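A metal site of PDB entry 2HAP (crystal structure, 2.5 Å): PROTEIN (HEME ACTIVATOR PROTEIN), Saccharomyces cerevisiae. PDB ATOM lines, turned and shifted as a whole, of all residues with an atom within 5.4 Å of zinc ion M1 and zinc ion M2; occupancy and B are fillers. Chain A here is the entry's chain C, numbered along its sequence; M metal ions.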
ATOM      1  N   ARG A   9      -3.729  -0.787   3.600  1.00  0.00           N
ATOM      2  CA  ARG A   9      -4.612   0.237   3.055  1.00  0.00           C
ATOM      3  C   ARG A   9      -5.978  -0.081   3.650  1.00  0.00           C
ATOM      4  O   ARG A   9      -6.348  -1.259   3.704  1.00  0.00           O
ATOM      5  CB  ARG A   9      -4.672   0.112   1.541  1.00  0.00           C
ATOM      6  CG  ARG A   9      -4.798  -1.304   1.055  1.00  0.00           C
ATOM      7  CD  ARG A   9      -5.107  -1.330  -0.422  1.00  0.00           C
ATOM      8  NE  ARG A   9      -5.095  -2.686  -0.928  1.00  0.00           N
ATOM      9  CZ  ARG A   9      -5.519  -3.026  -2.142  1.00  0.00           C
ATOM     10  NH1 ARG A   9      -5.974  -2.086  -2.956  1.00  0.00           N
ATOM     11  NH2 ARG A   9      -5.495  -4.294  -2.548  1.00  0.00           N
ATOM     12  N   CYS A  10      -6.713   0.930   4.123  1.00  0.00           N
ATOM     13  CA  CYS A  10      -8.033   0.695   4.712  1.00  0.00           C
ATOM     14  C   CYS A  10      -8.875  -0.132   3.718  1.00  0.00           C
ATOM     15  O   CYS A  10      -8.625  -0.142   2.498  1.00  0.00           O
ATOM     16  CB  CYS A  10      -8.736   2.017   5.046  1.00  0.00           C
ATOM     17  SG  CYS A  10      -9.434   2.758   3.558  1.00  0.00           S
ATOM     18  N   ILE A  12     -11.871   0.214   2.543  1.00  0.00           N
ATOM     19  CA  ILE A  12     -12.590   0.947   1.491  1.00  0.00           C
ATOM     20  C   ILE A  12     -11.650   1.223   0.324  1.00  0.00           C
ATOM     21  O   ILE A  12     -12.036   1.105  -0.842  1.00  0.00           O
ATOM     22  CB  ILE A  12     -13.142   2.297   2.005  1.00  0.00           C
ATOM     23  CG1 ILE A  12     -14.332   2.047   2.917  1.00  0.00           C
ATOM     24  CG2 ILE A  12     -13.588   3.177   0.832  1.00  0.00           C
ATOM     25  CD1 ILE A  12     -15.561   1.561   2.193  1.00  0.00           C
ATOM     26  N   CYS A  13     -10.403   1.570   0.637  1.00  0.00           N
ATOM     27  CA  CYS A  13      -9.447   1.848  -0.424  1.00  0.00           C
ATOM     28  C   CYS A  13      -9.154   0.595  -1.249  1.00  0.00           C
ATOM     29  O   CYS A  13      -9.011   0.669  -2.466  1.00  0.00           O
ATOM     30  CB  CYS A  13      -8.176   2.433   0.186  1.00  0.00           C
ATOM     31  SG  CYS A  13      -8.279   4.246   0.413  1.00  0.00           S
ATOM     32  N   LYS A  19      -5.108   4.477  -3.611  1.00  0.00           N
ATOM     33  CA  LYS A  19      -4.013   4.591  -2.644  1.00  0.00           C
ATOM     34  C   LYS A  19      -4.452   5.126  -1.299  1.00  0.00           C
ATOM     35  O   LYS A  19      -5.150   6.135  -1.228  1.00  0.00           O
ATOM     36  CB  LYS A  19      -2.911   5.514  -3.172  1.00  0.00           C
ATOM     37  CG  LYS A  19      -1.503   4.969  -2.999  1.00  0.00           C
ATOM     38  CD  LYS A  19      -0.857   5.366  -1.674  1.00  0.00           C
ATOM     39  CE  LYS A  19       0.297   4.402  -1.320  1.00  0.00           C
ATOM     40  NZ  LYS A  19       0.679   4.413   0.132  1.00  0.00           N
ATOM     41  N   CYS A  20      -4.029   4.436  -0.240  1.00  0.00           N
ATOM     42  CA  CYS A  20      -4.392   4.840   1.101  1.00  0.00           C
ATOM     43  C   CYS A  20      -3.236   5.523   1.846  1.00  0.00           C
ATOM     44  O   CYS A  20      -2.146   4.974   1.931  1.00  0.00           O
ATOM     45  CB  CYS A  20      -4.857   3.605   1.869  1.00  0.00           C
ATOM     46  SG  CYS A  20      -5.678   3.986   3.448  1.00  0.00           S
ATOM     47  N   ASP A  21      -3.472   6.721   2.370  1.00  0.00           N
ATOM     48  CA  ASP A  21      -2.431   7.404   3.132  1.00  0.00           C
ATOM     49  C   ASP A  21      -2.315   6.757   4.508  1.00  0.00           C
ATOM     50  O   ASP A  21      -1.691   7.287   5.419  1.00  0.00           O
ATOM     51  CB  ASP A  21      -2.710   8.907   3.266  1.00  0.00           C
ATOM     52  CG  ASP A  21      -4.071   9.204   3.837  1.00  0.00           C
ATOM     53  OD1 ASP A  21      -4.425   8.594   4.876  1.00  0.00           O
ATOM     54  OD2 ASP A  21      -4.770  10.043   3.225  1.00  0.00           O
ATOM     55  N   HIS A  26      -8.925   7.358  10.487  1.00  0.00           N
ATOM     56  CA  HIS A  26      -9.462   7.120   9.160  1.00  0.00           C
ATOM     57  C   HIS A  26      -8.564   7.743   8.101  1.00  0.00           C
ATOM     58  O   HIS A  26      -8.137   8.873   8.247  1.00  0.00           O
ATOM     59  CB  HIS A  26     -10.869   7.687   9.039  1.00  0.00           C
ATOM     60  CG  HIS A  26     -11.766   7.380  10.212  1.00  0.00           C
ATOM     61  ND1 HIS A  26     -12.047   6.085  10.610  1.00  0.00           N
ATOM     62  CD2 HIS A  26     -12.416   8.196  11.064  1.00  0.00           C
ATOM     63  CE1 HIS A  26     -12.832   6.126  11.667  1.00  0.00           C
ATOM     64  NE2 HIS A  26     -13.071   7.388  11.962  1.00  0.00           N
ATOM     65  N   CYS A  27      -8.306   6.991   7.032  1.00  0.00           N
ATOM     66  CA  CYS A  27      -7.478   7.499   5.948  1.00  0.00           C
ATOM     67  C   CYS A  27      -8.180   8.716   5.347  1.00  0.00           C
ATOM     68  O   CYS A  27      -9.415   8.809   5.373  1.00  0.00           O
ATOM     69  CB  CYS A  27      -7.272   6.420   4.908  1.00  0.00           C
ATOM     70  SG  CYS A  27      -8.672   6.314   3.794  1.00  0.00           S
ATOM     71  N   GLN A  29      -8.435   9.490   2.215  1.00  0.00           N
ATOM     72  CA  GLN A  29      -9.118   9.210   0.962  1.00  0.00           C
ATOM     73  C   GLN A  29     -10.584   9.126   1.331  1.00  0.00           C
ATOM     74  O   GLN A  29     -11.422   9.800   0.732  1.00  0.00           O
ATOM     75  CB  GLN A  29      -8.653   7.889   0.359  1.00  0.00           C
ATOM     76  CG  GLN A  29      -7.267   7.938  -0.257  1.00  0.00           C
ATOM     77  CD  GLN A  29      -6.171   8.452   0.703  1.00  0.00           C
ATOM     78  OE1 GLN A  29      -6.041   7.976   1.840  1.00  0.00           O
ATOM     79  NE2 GLN A  29      -5.390   9.412   0.247  1.00  0.00           N
ATOM     80  N   CYS A  30     -10.894   8.302   2.333  1.00  0.00           N
ATOM     81  CA  CYS A  30     -12.264   8.133   2.793  1.00  0.00           C
ATOM     82  C   CYS A  30     -12.854   9.454   3.282  1.00  0.00           C
ATOM     83  O   CYS A  30     -13.970   9.800   2.923  1.00  0.00           O
ATOM     84  CB  CYS A  30     -12.344   7.096   3.925  1.00  0.00           C
ATOM     85  SG  CYS A  30     -12.177   5.357   3.387  1.00  0.00           S
ATOM     86  N   CYS A  39     -14.456   3.762   7.116  1.00  0.00           N
ATOM     87  CA  CYS A  39     -13.027   3.444   7.018  1.00  0.00           C
ATOM     88  C   CYS A  39     -12.673   2.491   8.132  1.00  0.00           C
ATOM     89  O   CYS A  39     -13.093   2.677   9.276  1.00  0.00           O
ATOM     90  CB  CYS A  39     -12.184   4.736   7.164  1.00  0.00           C
ATOM     91  SG  CYS A  39     -10.404   4.582   6.735  1.00  0.00           S
ATOM     92  N   HIS A  40     -11.888   1.463   7.814  1.00  0.00           N
ATOM     93  CA  HIS A  40     -11.486   0.477   8.818  1.00  0.00           C
ATOM     94  C   HIS A  40     -10.241  -0.274   8.334  1.00  0.00           C
ATOM     95  O   HIS A  40     -10.121  -0.593   7.159  1.00  0.00           O
ATOM     96  CB  HIS A  40     -12.665  -0.479   9.122  1.00  0.00           C
ATOM     97  CG  HIS A  40     -12.276  -1.921   9.307  1.00  0.00           C
ATOM     98  ND1 HIS A  40     -11.809  -2.419  10.505  1.00  0.00           N
ATOM     99  CD2 HIS A  40     -12.266  -2.953   8.434  1.00  0.00           C
ATOM    100  CE1 HIS A  40     -11.519  -3.697  10.364  1.00  0.00           C
ATOM    101  NE2 HIS A  40     -11.776  -4.053   9.117  1.00  0.00           N
ATOM    102  N   TYR A  41      -9.305  -0.527   9.240  1.00  0.00           N
ATOM    103  CA  TYR A  41      -8.098  -1.270   8.900  1.00  0.00           C
ATOM    104  C   TYR A  41      -8.160  -2.669   9.488  1.00  0.00           C
ATOM    105  O   TYR A  41      -8.499  -2.833  10.663  1.00  0.00           O
ATOM    106  CB  TYR A  41      -6.835  -0.543   9.431  1.00  0.00           C
ATOM    107  CG  TYR A  41      -6.594   0.820   8.810  1.00  0.00           C
ATOM    108  CD1 TYR A  41      -6.044   0.939   7.530  1.00  0.00           C
ATOM    109  CD2 TYR A  41      -6.993   1.990   9.464  1.00  0.00           C
ATOM    110  CE1 TYR A  41      -5.883   2.183   6.931  1.00  0.00           C
ATOM    111  CE2 TYR A  41      -6.835   3.226   8.877  1.00  0.00           C
ATOM    112  CZ  TYR A  41      -6.295   3.324   7.606  1.00  0.00           C
ATOM    113  OH  TYR A  41      -6.190   4.554   6.983  1.00  0.00           O
HETATM  114 ZN    ZN M   1      -7.941   4.456   2.667  1.00  0.00          ZN
HETATM  115 ZN    ZN M   2     -10.254   4.670   4.468  1.00  0.00          ZN
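The side-chain sulfur (SG) of Cys 10 sits close to the backbone NH (N) of Ile 12 (3.7 Å).
The side-chain sulfur (SG) of Cys 27 lies close to the backbone NH (N) of Gln 29 (3.6 Å).
N of Cys 27 sits close to OH of Tyr 41 (3.2 Å).
The side-chain hydroxyl of Tyr 41 lies close to the side-chain sulfur of Cys 20.
Within 4 Å of zinc ion M1: Cys 10, Cys 13, Cys 20 and Cys 27.
The nearest printed residue that does not touch zinc ion M1 is Gln 29 (4.1 Å).
Four residues have an atom within 4 Å of zinc ion M2: Cys 10, Cys 27, Cys 30 and Cys 39.
Zinc ion M1 is bound by the side-chain sulfur of Cys 13, the side-chain sulfur of Cys 27, the side-chain sulfur of Cys 10 and the side-chain sulfur of Cys 20.
Zinc ion M2 is bound by SG of Cys 10 (2.3 Å), SG of Cys 39 (2.3 Å), SG of Cys 30 (2.3 Å) and SG of Cys 27 (2.4 Å).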
